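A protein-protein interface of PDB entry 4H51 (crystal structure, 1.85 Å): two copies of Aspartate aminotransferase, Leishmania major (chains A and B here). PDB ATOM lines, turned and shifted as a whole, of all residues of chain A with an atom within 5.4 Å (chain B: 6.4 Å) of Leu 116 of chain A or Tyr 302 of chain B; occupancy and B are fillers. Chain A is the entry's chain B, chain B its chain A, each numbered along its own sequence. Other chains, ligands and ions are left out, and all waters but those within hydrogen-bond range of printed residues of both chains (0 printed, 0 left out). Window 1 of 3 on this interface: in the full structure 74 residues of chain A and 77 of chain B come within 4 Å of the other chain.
Of the 15 printed residues of chain A, 6 touch a printed residue of chain B.
Hydrophobic or aromatic side chains of chain B that line the printed part of chain A: Leu 116, Tyr 302 and Pro 306.
Along chain B the printed residues that touch a printed residue of chain A span positions 116 to 306.
Among the printed residues, no Asp or Glu carboxylate lies within 4 Å of a Lys or Arg side-chain nitrogen of the other chain.
Leu 116 of chain A touches Leu 116 of chain B (CD1 to CD2, 3.9 Å).
CB of Leu 116 of chain A touches CB of Tyr 302 of chain B, 3.8 Å away.
Thr 119 of chain A touches Glu 301 of chain B.
CG2 of Thr 119 of chain A touches CA of Tyr 302 of chain B, 3.7 Å away.
Glu 301 of chain B touches Gly 120 of chain A (O to CA, 3.6 Å).
Arg 273 of chain A touches Thr 303 of chain B.
CG of Arg 273 of chain A touches C of Pro 305 of chain B, 3.8 Å away.
CG of Arg 273 of chain A touches N of Pro 306 of chain B, 3.6 Å away.
Tyr 302 of chain A touches Leu 116 of chain B.
Pro 306 of chain A touches Pro 306 of chain B (CG to CG, 3.8 Å).
Of the printed residues of chain B, Leu 116 of chain A touches Leu 116 and Tyr 302.
Of the printed residues of chain B, Gly 120 of chain A touches Glu 301.
Printed residues of chain B within 4 Å of Arg 273 of chain A: Tyr 302 (2.8 Å), Thr 303 (3.7 Å), Cys 304 (2.9 Å), Pro 305 (3.8 Å) and Pro 306 (3.6 Å).
Of the printed residues of chain B, Pro 306 of chain A touches Pro 306.
Leu 124 of chain B touches none of the printed residues of chain A.
Of the printed residues of chain A, Arg 299 of chain B touches Thr 119 (3.9 Å).
Of the printed residues of chain A, Tyr 302 of chain B touches Leu 116, Thr 119 and Arg 273.
The nearest printed residue of chain B that does not touch Leu 116 of chain A is Pro 306 of chain B (4.2 Å).
The nearest printed residue of chain B that does not touch Pro 306 of chain A is Leu 116 of chain B (5.7 Å).
The guanidinium group (NH2) of Arg 273 of chain A lies within hydrogen-bond range of the backbone carbonyl oxygen (O) of Tyr 302 of chain B.
OG1 of Thr 303 of chain B sits at hydrogen-bond distance from OG1 of Thr 119 of chain A, 2.8 Å away.
O of Cys 304 of chain B is in hydrogen-bond range of NE of Arg 273 of chain A (2.9 Å).
Leu 116 of chain A touches its own counterpart, Leu 116 of chain B.
Leu 116 of chain A touches Tyr 302 of chain B, and with the chains exchanged Tyr 302 of chain A touches Leu 116 of chain B.
Pro 306 of chain B touches its own counterpart, Pro 306 of chain A.
7 positions are printed for both chains.
Of the 14 pairs that touch across the chains among the printed residues, 4 have their exchanged pair printed and touching as well.
The side-chain amide nitrogen (NE2) of Gln 114 of chain B lies within hydrogen-bond range of the backbone carbonyl oxygen (O) of Pro 306 of chain B (2.9 Å).
O of Ile 298 of chain B is in hydrogen-bond range of N of Thr 303 of chain B (3.2 Å).
The side-chain amide nitrogen (NE2) of Gln 114 of chain A sits at hydrogen-bond distance from the backbone carbonyl oxygen (O) of Pro 306 of chain A (2.9 Å).
The backbone carbonyl oxygen (O) of Arg 273 of chain A sits at hydrogen-bond distance from the backbone NH (N) of Ser 117 of chain A (3.2 Å).
The side-chain hydroxyl (OG1) of Thr 119 of chain A is in hydrogen-bond range of OP1 of LLP 265 of chain A, at 2.6 Å.
NH1 of Arg 273 of chain A lies close to OP2 of LLP 265 of chain A (2.9 Å).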
ATOM      1  N   GLN A 114      16.389  10.011 -14.761  1.00  0.00           N
ATOM      2  CA  GLN A 114      16.066   9.079 -15.817  1.00  0.00           C
ATOM      3  C   GLN A 114      15.009   8.083 -15.314  1.00  0.00           C
ATOM      4  O   GLN A 114      15.034   7.649 -14.151  1.00  0.00           O
ATOM      5  CB  GLN A 114      17.360   8.364 -16.306  1.00  0.00           C
ATOM      6  CG  GLN A 114      17.133   7.326 -17.385  1.00  0.00           C
ATOM      7  CD  GLN A 114      18.382   6.652 -17.822  1.00  0.00           C
ATOM      8  OE1 GLN A 114      19.459   7.203 -17.621  1.00  0.00           O
ATOM      9  NE2 GLN A 114      18.256   5.466 -18.472  1.00  0.00           N
ATOM     10  N   THR A 115      14.090   7.717 -16.183  1.00  0.00           N
ATOM     11  CA  THR A 115      13.000   6.810 -15.853  1.00  0.00           C
ATOM     12  C   THR A 115      12.871   5.706 -16.891  1.00  0.00           C
ATOM     13  O   THR A 115      13.472   5.770 -17.953  1.00  0.00           O
ATOM     14  CB  THR A 115      11.656   7.569 -15.821  1.00  0.00           C
ATOM     15  OG1 THR A 115      11.430   8.163 -17.136  1.00  0.00           O
ATOM     16  CG2 THR A 115      11.667   8.659 -14.704  1.00  0.00           C
ATOM     17  N   LEU A 116      12.030   4.707 -16.590  1.00  0.00           N
ATOM     18  CA  LEU A 116      11.702   3.674 -17.569  1.00  0.00           C
ATOM     19  C   LEU A 116      10.706   4.233 -18.594  1.00  0.00           C
ATOM     20  O   LEU A 116       9.523   3.909 -18.589  1.00  0.00           O
ATOM     21  CB  LEU A 116      11.174   2.407 -16.887  1.00  0.00           C
ATOM     22  CG  LEU A 116      12.249   1.375 -16.502  1.00  0.00           C
ATOM     23  CD1 LEU A 116      12.851   0.748 -17.757  1.00  0.00           C
ATOM     24  CD2 LEU A 116      13.349   1.936 -15.583  1.00  0.00           C
ATOM     25  N   SER A 117      11.211   5.077 -19.480  1.00  0.00           N
ATOM     26  CA  SER A 117      10.425   5.721 -20.508  1.00  0.00           C
ATOM     27  C   SER A 117       9.331   6.606 -19.891  1.00  0.00           C
ATOM     28  O   SER A 117       9.390   6.941 -18.685  1.00  0.00           O
ATOM     29  CB  SER A 117       9.874   4.673 -21.489  1.00  0.00           C
ATOM     30  OG  SER A 117      10.060   5.158 -22.819  1.00  0.00           O
ATOM     31  N   GLY A 118       8.331   6.947 -20.681  1.00  0.00           N
ATOM     32  CA  GLY A 118       7.261   7.817 -20.221  1.00  0.00           C
ATOM     33  C   GLY A 118       6.343   7.147 -19.242  1.00  0.00           C
ATOM     34  O   GLY A 118       5.836   7.782 -18.341  1.00  0.00           O
ATOM     35  N   THR A 119       6.088   5.856 -19.420  1.00  0.00           N
ATOM     36  CA  THR A 119       5.229   5.154 -18.488  1.00  0.00           C
ATOM     37  C   THR A 119       5.910   5.200 -17.126  1.00  0.00           C
ATOM     38  O   THR A 119       5.278   5.527 -16.140  1.00  0.00           O
ATOM     39  CB  THR A 119       4.956   3.678 -18.862  1.00  0.00           C
ATOM     40  OG1 THR A 119       4.424   3.554 -20.199  1.00  0.00           O
ATOM     41  CG2 THR A 119       4.024   3.019 -17.817  1.00  0.00           C
ATOM     42  N   GLY A 120       7.194   4.856 -17.083  1.00  0.00           N
ATOM     43  CA  GLY A 120       7.972   4.884 -15.841  1.00  0.00           C
ATOM     44  C   GLY A 120       7.929   6.248 -15.185  1.00  0.00           C
ATOM     45  O   GLY A 120       7.851   6.376 -13.949  1.00  0.00           O
ATOM     46  N   ALA A 121       8.022   7.303 -15.997  1.00  0.00           N
ATOM     47  CA  ALA A 121       7.974   8.661 -15.455  1.00  0.00           C
ATOM     48  C   ALA A 121       6.601   9.029 -14.890  1.00  0.00           C
ATOM     49  O   ALA A 121       6.517   9.742 -13.877  1.00  0.00           O
ATOM     50  CB  ALA A 121       8.417   9.668 -16.558  1.00  0.00           C
ATOM     51  N1  LLP A 265       1.687   8.637 -22.183  1.00  0.00           N
ATOM     52  C2  LLP A 265       0.913   8.640 -23.284  1.00  0.00           C
ATOM     53  C2' LLP A 265      -0.368   9.440 -23.309  1.00  0.00           C
ATOM     54  C3  LLP A 265       1.340   7.889 -24.478  1.00  0.00           C
ATOM     55  O3  LLP A 265       0.607   7.860 -25.617  1.00  0.00           O
ATOM     56  C4  LLP A 265       2.625   7.186 -24.442  1.00  0.00           C
ATOM     57  C4' LLP A 265       2.971   6.446 -25.692  1.00  0.00           C
ATOM     58  C5  LLP A 265       3.369   7.203 -23.156  1.00  0.00           C
ATOM     59  C6  LLP A 265       2.836   7.962 -22.102  1.00  0.00           C
ATOM     60  C5' LLP A 265       4.752   6.570 -22.923  1.00  0.00           C
ATOM     61  OP4 LLP A 265       5.063   5.339 -23.542  1.00  0.00           O
ATOM     62  P   LLP A 265       6.506   4.766 -23.187  1.00  0.00           P
ATOM     63  OP1 LLP A 265       6.314   4.230 -21.786  1.00  0.00           O
ATOM     64  OP2 LLP A 265       6.802   3.786 -24.255  1.00  0.00           O
ATOM     65  OP3 LLP A 265       7.488   5.968 -23.133  1.00  0.00           O
ATOM     66  N   LLP A 265       8.662   7.345 -29.090  1.00  0.00           N
ATOM     67  CA  LLP A 265       8.045   7.714 -30.368  1.00  0.00           C
ATOM     68  CB  LLP A 265       6.677   8.321 -30.112  1.00  0.00           C
ATOM     69  CG  LLP A 265       5.768   7.186 -29.621  1.00  0.00           C
ATOM     70  CD  LLP A 265       5.498   7.414 -28.161  1.00  0.00           C
ATOM     71  CE  LLP A 265       4.544   6.364 -27.622  1.00  0.00           C
ATOM     72  NZ  LLP A 265       4.201   6.823 -26.293  1.00  0.00           N
ATOM     73  C   LLP A 265       8.922   8.641 -31.174  1.00  0.00           C
ATOM     74  O   LLP A 265       9.104   8.392 -32.361  1.00  0.00           O
ATOM     75  N   ARG A 273      13.216   1.983 -23.640  1.00  0.00           N
ATOM     76  CA  ARG A 273      12.601   2.539 -22.454  1.00  0.00           C
ATOM     77  C   ARG A 273      13.382   3.725 -21.885  1.00  0.00           C
ATOM     78  O   ARG A 273      13.777   3.721 -20.714  1.00  0.00           O
ATOM     79  CB  ARG A 273      12.416   1.475 -21.368  1.00  0.00           C
ATOM     80  CG  ARG A 273      12.056   0.054 -21.844  1.00  0.00           C
ATOM     81  CD  ARG A 273      10.803  -0.043 -22.670  1.00  0.00           C
ATOM     82  NE  ARG A 273       9.602   0.415 -21.940  1.00  0.00           N
ATOM     83  CZ  ARG A 273       8.763   1.364 -22.321  1.00  0.00           C
ATOM     84  NH1 ARG A 273       8.954   2.016 -23.478  1.00  0.00           N
ATOM     85  NH2 ARG A 273       7.747   1.695 -21.523  1.00  0.00           N
ATOM     86  N   ALA A 274      13.550   4.759 -22.698  1.00  0.00           N
ATOM     87  CA  ALA A 274      14.339   5.950 -22.303  1.00  0.00           C
ATOM     88  C   ALA A 274      13.385   7.109 -22.054  1.00  0.00           C
ATOM     89  O   ALA A 274      12.664   7.549 -22.967  1.00  0.00           O
ATOM     90  CB  ALA A 274      15.351   6.322 -23.383  1.00  0.00           C
ATOM     91  N   GLY A 275      13.403   7.618 -20.831  1.00  0.00           N
ATOM     92  CA  GLY A 275      12.508   8.712 -20.428  1.00  0.00           C
ATOM     93  C   GLY A 275      13.119   9.526 -19.307  1.00  0.00           C
ATOM     94  O   GLY A 275      14.146   9.143 -18.736  1.00  0.00           O
ATOM     95  N   TYR A 302      13.653  -0.773  -8.782  1.00  0.00           N
ATOM     96  CA  TYR A 302      14.499  -1.396  -9.779  1.00  0.00           C
ATOM     97  C   TYR A 302      15.959  -0.969  -9.653  1.00  0.00           C
ATOM     98  O   TYR A 302      16.739  -1.292 -10.497  1.00  0.00           O
ATOM     99  CB  TYR A 302      13.966  -1.138 -11.186  1.00  0.00           C
ATOM    100  CG  TYR A 302      13.874   0.305 -11.583  1.00  0.00           C
ATOM    101  CD1 TYR A 302      14.954   0.971 -12.131  1.00  0.00           C
ATOM    102  CD2 TYR A 302      12.713   1.039 -11.336  1.00  0.00           C
ATOM    103  CE1 TYR A 302      14.873   2.312 -12.475  1.00  0.00           C
ATOM    104  CE2 TYR A 302      12.611   2.394 -11.684  1.00  0.00           C
ATOM    105  CZ  TYR A 302      13.701   3.036 -12.218  1.00  0.00           C
ATOM    106  OH  TYR A 302      13.624   4.377 -12.569  1.00  0.00           O
ATOM    107  N   PRO A 305      18.322   2.639 -13.752  1.00  0.00           N
ATOM    108  CA  PRO A 305      17.680   2.418 -15.044  1.00  0.00           C
ATOM    109  C   PRO A 305      18.591   1.805 -16.111  1.00  0.00           C
ATOM    110  O   PRO A 305      19.834   1.872 -15.976  1.00  0.00           O
ATOM    111  CB  PRO A 305      17.262   3.829 -15.461  1.00  0.00           C
ATOM    112  CG  PRO A 305      18.373   4.676 -14.922  1.00  0.00           C
ATOM    113  CD  PRO A 305      18.798   4.041 -13.613  1.00  0.00           C
ATOM    114  N   PRO A 306      17.987   1.245 -17.183  1.00  0.00           N
ATOM    115  CA  PRO A 306      18.759   0.680 -18.289  1.00  0.00           C
ATOM    116  C   PRO A 306      19.503   1.771 -19.087  1.00  0.00           C
ATOM    117  O   PRO A 306      18.940   2.823 -19.382  1.00  0.00           O
ATOM    118  CB  PRO A 306      17.718  -0.050 -19.155  1.00  0.00           C
ATOM    119  CG  PRO A 306      16.429   0.667 -18.857  1.00  0.00           C
ATOM    120  CD  PRO A 306      16.530   1.182 -17.429  1.00  0.00           C
ATOM    121  N   ILE B  86       4.442  -7.144 -22.837  1.00  0.00           N
ATOM    122  CA  ILE B  86       4.513  -6.716 -21.426  1.00  0.00           C
ATOM    123  C   ILE B  86       5.414  -7.641 -20.610  1.00  0.00           C
ATOM    124  O   ILE B  86       6.228  -7.206 -19.786  1.00  0.00           O
ATOM    125  CB  ILE B  86       3.100  -6.663 -20.815  1.00  0.00           C
ATOM    126  CG1 ILE B  86       2.281  -5.551 -21.466  1.00  0.00           C
ATOM    127  CG2 ILE B  86       3.150  -6.469 -19.298  1.00  0.00           C
ATOM    128  CD1 ILE B  86       0.787  -5.652 -21.165  1.00  0.00           C
ATOM    129  N   VAL B 113       8.172 -14.130 -16.208  1.00  0.00           N
ATOM    130  CA  VAL B 113       8.339 -12.895 -16.999  1.00  0.00           C
ATOM    131  C   VAL B 113       9.734 -12.273 -16.857  1.00  0.00           C
ATOM    132  O   VAL B 113      10.450 -12.572 -15.909  1.00  0.00           O
ATOM    133  CB  VAL B 113       7.312 -11.830 -16.536  1.00  0.00           C
ATOM    134  CG1 VAL B 113       5.864 -12.343 -16.732  1.00  0.00           C
ATOM    135  CG2 VAL B 113       7.557 -11.469 -15.070  1.00  0.00           C
ATOM    136  N   GLN B 114      10.097 -11.429 -17.825  1.00  0.00           N
ATOM    137  CA  GLN B 114      11.312 -10.638 -17.784  1.00  0.00           C
ATOM    138  C   GLN B 114      11.065  -9.490 -16.802  1.00  0.00           C
ATOM    139  O   GLN B 114       9.930  -8.999 -16.706  1.00  0.00           O
ATOM    140  CB  GLN B 114      11.580 -10.092 -19.181  1.00  0.00           C
ATOM    141  CG  GLN B 114      12.827  -9.232 -19.264  1.00  0.00           C
ATOM    142  CD  GLN B 114      13.101  -8.729 -20.667  1.00  0.00           C
ATOM    143  OE1 GLN B 114      12.678  -9.353 -21.664  1.00  0.00           O
ATOM    144  NE2 GLN B 114      13.870  -7.613 -20.771  1.00  0.00           N
ATOM    145  N   THR B 115      12.080  -9.106 -16.058  1.00  0.00           N
ATOM    146  CA  THR B 115      11.949  -8.056 -15.066  1.00  0.00           C
ATOM    147  C   THR B 115      13.106  -7.090 -15.223  1.00  0.00           C
ATOM    148  O   THR B 115      13.999  -7.377 -15.968  1.00  0.00           O
ATOM    149  CB  THR B 115      11.995  -8.630 -13.671  1.00  0.00           C
ATOM    150  OG1 THR B 115      13.229  -9.355 -13.489  1.00  0.00           O
ATOM    151  CG2 THR B 115      10.794  -9.562 -13.443  1.00  0.00           C
ATOM    152  N   LEU B 116      13.043  -5.962 -14.504  1.00  0.00           N
ATOM    153  CA  LEU B 116      14.147  -5.012 -14.443  1.00  0.00           C
ATOM    154  C   LEU B 116      15.225  -5.578 -13.521  1.00  0.00           C
ATOM    155  O   LEU B 116      15.440  -5.103 -12.359  1.00  0.00           O
ATOM    156  CB  LEU B 116      13.631  -3.638 -13.975  1.00  0.00           C
ATOM    157  CG  LEU B 116      12.433  -3.125 -14.829  1.00  0.00           C
ATOM    158  CD1 LEU B 116      11.793  -1.875 -14.295  1.00  0.00           C
ATOM    159  CD2 LEU B 116      12.804  -2.914 -16.300  1.00  0.00           C
ATOM    160  N   GLY B 120      14.197  -5.596  -9.782  1.00  0.00           N
ATOM    161  CA  GLY B 120      12.823  -5.576 -10.316  1.00  0.00           C
ATOM    162  C   GLY B 120      12.072  -6.873 -10.060  1.00  0.00           C
ATOM    163  O   GLY B 120      10.864  -6.852  -9.764  1.00  0.00           O
ATOM    164  N   LEU B 124       8.654  -7.080  -8.009  1.00  0.00           N
ATOM    165  CA  LEU B 124       7.450  -7.602  -8.660  1.00  0.00           C
ATOM    166  C   LEU B 124       6.939  -8.856  -7.905  1.00  0.00           C
ATOM    167  O   LEU B 124       5.731  -9.028  -7.698  1.00  0.00           O
ATOM    168  CB  LEU B 124       7.735  -7.971 -10.111  1.00  0.00           C
ATOM    169  CG  LEU B 124       6.587  -8.562 -10.915  1.00  0.00           C
ATOM    170  CD1 LEU B 124       5.445  -7.572 -11.046  1.00  0.00           C
ATOM    171  CD2 LEU B 124       7.066  -8.975 -12.317  1.00  0.00           C
ATOM    172  N   LEU B 297       0.680  -5.911 -13.170  1.00  0.00           N
ATOM    173  CA  LEU B 297       1.611  -5.182 -12.326  1.00  0.00           C
ATOM    174  C   LEU B 297       2.713  -4.484 -13.157  1.00  0.00           C
ATOM    175  O   LEU B 297       3.129  -3.334 -12.861  1.00  0.00           O
ATOM    176  CB  LEU B 297       2.266  -6.119 -11.297  1.00  0.00           C
ATOM    177  CG  LEU B 297       1.350  -6.560 -10.160  1.00  0.00           C
ATOM    178  CD1 LEU B 297       1.946  -7.739  -9.407  1.00  0.00           C
ATOM    179  CD2 LEU B 297       1.107  -5.377  -9.229  1.00  0.00           C
ATOM    180  N   ILE B 298       3.234  -5.193 -14.144  1.00  0.00           N
ATOM    181  CA  ILE B 298       4.225  -4.583 -15.054  1.00  0.00           C
ATOM    182  C   ILE B 298       3.639  -3.403 -15.834  1.00  0.00           C
ATOM    183  O   ILE B 298       4.248  -2.313 -15.890  1.00  0.00           O
ATOM    184  CB  ILE B 298       4.792  -5.595 -16.044  1.00  0.00           C
ATOM    185  CG1 ILE B 298       5.593  -6.666 -15.311  1.00  0.00           C
ATOM    186  CG2 ILE B 298       5.659  -4.901 -17.102  1.00  0.00           C
ATOM    187  CD1 ILE B 298       5.748  -7.979 -16.111  1.00  0.00           C
ATOM    188  N   ARG B 299       2.440  -3.582 -16.383  1.00  0.00           N
ATOM    189  CA  ARG B 299       1.870  -2.578 -17.274  1.00  0.00           C
ATOM    190  C   ARG B 299       1.667  -1.241 -16.541  1.00  0.00           C
ATOM    191  O   ARG B 299       1.951  -0.170 -17.086  1.00  0.00           O
ATOM    192  CB  ARG B 299       0.553  -3.093 -17.848  1.00  0.00           C
ATOM    193  CG  ARG B 299      -0.270  -2.201 -18.773  1.00  0.00           C
ATOM    194  CD  ARG B 299       0.472  -1.470 -19.878  1.00  0.00           C
ATOM    195  NE  ARG B 299      -0.444  -1.147 -20.986  1.00  0.00           N
ATOM    196  CZ  ARG B 299      -0.225  -0.236 -21.942  1.00  0.00           C
ATOM    197  NH1 ARG B 299       0.878   0.526 -21.933  1.00  0.00           N
ATOM    198  NH2 ARG B 299      -1.148  -0.080 -22.903  1.00  0.00           N
ATOM    199  N   GLU B 300       1.238  -1.335 -15.292  1.00  0.00           N
ATOM    200  CA  GLU B 300       0.951  -0.182 -14.483  1.00  0.00           C
ATOM    201  C   GLU B 300       2.178   0.505 -13.890  1.00  0.00           C
ATOM    202  O   GLU B 300       2.043   1.585 -13.275  1.00  0.00           O
ATOM    203  CB  GLU B 300      -0.080  -0.574 -13.382  1.00  0.00           C
ATOM    204  CG  GLU B 300       0.475  -1.314 -12.160  1.00  0.00           C
ATOM    205  CD  GLU B 300      -0.577  -2.059 -11.325  1.00  0.00           C
ATOM    206  OE1 GLU B 300      -0.228  -2.494 -10.247  1.00  0.00           O
ATOM    207  OE2 GLU B 300      -1.756  -2.156 -11.712  1.00  0.00           O
ATOM    208  N   GLU B 301       3.362  -0.076 -14.082  1.00  0.00           N
ATOM    209  CA  GLU B 301       4.594   0.526 -13.601  1.00  0.00           C
ATOM    210  C   GLU B 301       5.422   1.038 -14.782  1.00  0.00           C
ATOM    211  O   GLU B 301       5.836   2.208 -14.787  1.00  0.00           O
ATOM    212  CB  GLU B 301       5.417  -0.444 -12.722  1.00  0.00           C
ATOM    213  N   TYR B 302       5.714   0.191 -15.774  1.00  0.00           N
ATOM    214  CA  TYR B 302       6.662   0.593 -16.830  1.00  0.00           C
ATOM    215  C   TYR B 302       6.331   0.085 -18.259  1.00  0.00           C
ATOM    216  O   TYR B 302       7.123   0.271 -19.164  1.00  0.00           O
ATOM    217  CB  TYR B 302       8.116   0.226 -16.417  1.00  0.00           C
ATOM    218  CG  TYR B 302       8.351  -1.272 -16.196  1.00  0.00           C
ATOM    219  CD1 TYR B 302       8.690  -2.089 -17.266  1.00  0.00           C
ATOM    220  CD2 TYR B 302       8.203  -1.853 -14.931  1.00  0.00           C
ATOM    221  CE1 TYR B 302       8.898  -3.454 -17.101  1.00  0.00           C
ATOM    222  CE2 TYR B 302       8.414  -3.213 -14.736  1.00  0.00           C
ATOM    223  CZ  TYR B 302       8.743  -4.018 -15.818  1.00  0.00           C
ATOM    224  OH  TYR B 302       8.949  -5.382 -15.661  1.00  0.00           O
ATOM    225  N   THR B 303       5.144  -0.511 -18.404  1.00  0.00           N
ATOM    226  CA  THR B 303       4.552  -0.973 -19.678  1.00  0.00           C
ATOM    227  C   THR B 303       5.214  -2.248 -20.181  1.00  0.00           C
ATOM    228  O   THR B 303       4.539  -3.285 -20.313  1.00  0.00           O
ATOM    229  CB  THR B 303       4.471   0.119 -20.746  1.00  0.00           C
ATOM    230  OG1 THR B 303       3.394   1.003 -20.402  1.00  0.00           O
ATOM    231  CG2 THR B 303       4.183  -0.476 -22.180  1.00  0.00           C
ATOM    232  N   CYS B 304       6.527  -2.206 -20.429  1.00  0.00           N
ATOM    233  CA  CYS B 304       7.232  -3.394 -20.903  1.00  0.00           C
ATOM    234  C   CYS B 304       8.741  -3.186 -20.699  1.00  0.00           C
ATOM    235  O   CYS B 304       9.173  -2.037 -20.505  1.00  0.00           O
ATOM    236  CB  CYS B 304       6.879  -3.707 -22.350  1.00  0.00           C
ATOM    237  SG  CYS B 304       7.249  -2.346 -23.490  1.00  0.00           S
ATOM    238  N   PRO B 305       9.529  -4.267 -20.705  1.00  0.00           N
ATOM    239  CA  PRO B 305      10.921  -4.112 -20.227  1.00  0.00           C
ATOM    240  C   PRO B 305      11.869  -3.744 -21.330  1.00  0.00           C
ATOM    241  O   PRO B 305      11.540  -3.912 -22.502  1.00  0.00           O
ATOM    242  CB  PRO B 305      11.263  -5.493 -19.663  1.00  0.00           C
ATOM    243  CG  PRO B 305      10.472  -6.433 -20.536  1.00  0.00           C
ATOM    244  CD  PRO B 305       9.190  -5.681 -20.918  1.00  0.00           C
ATOM    245  N   PRO B 306      13.076  -3.294 -20.970  1.00  0.00           N
ATOM    246  CA  PRO B 306      14.056  -2.986 -22.002  1.00  0.00           C
ATOM    247  C   PRO B 306      14.620  -4.234 -22.682  1.00  0.00           C
ATOM    248  O   PRO B 306      14.903  -5.225 -21.997  1.00  0.00           O
ATOM    249  CB  PRO B 306      15.174  -2.277 -21.225  1.00  0.00           C
ATOM    250  CG  PRO B 306      15.018  -2.718 -19.838  1.00  0.00           C
ATOM    251  CD  PRO B 306      13.563  -2.947 -19.612  1.00  0.00           C
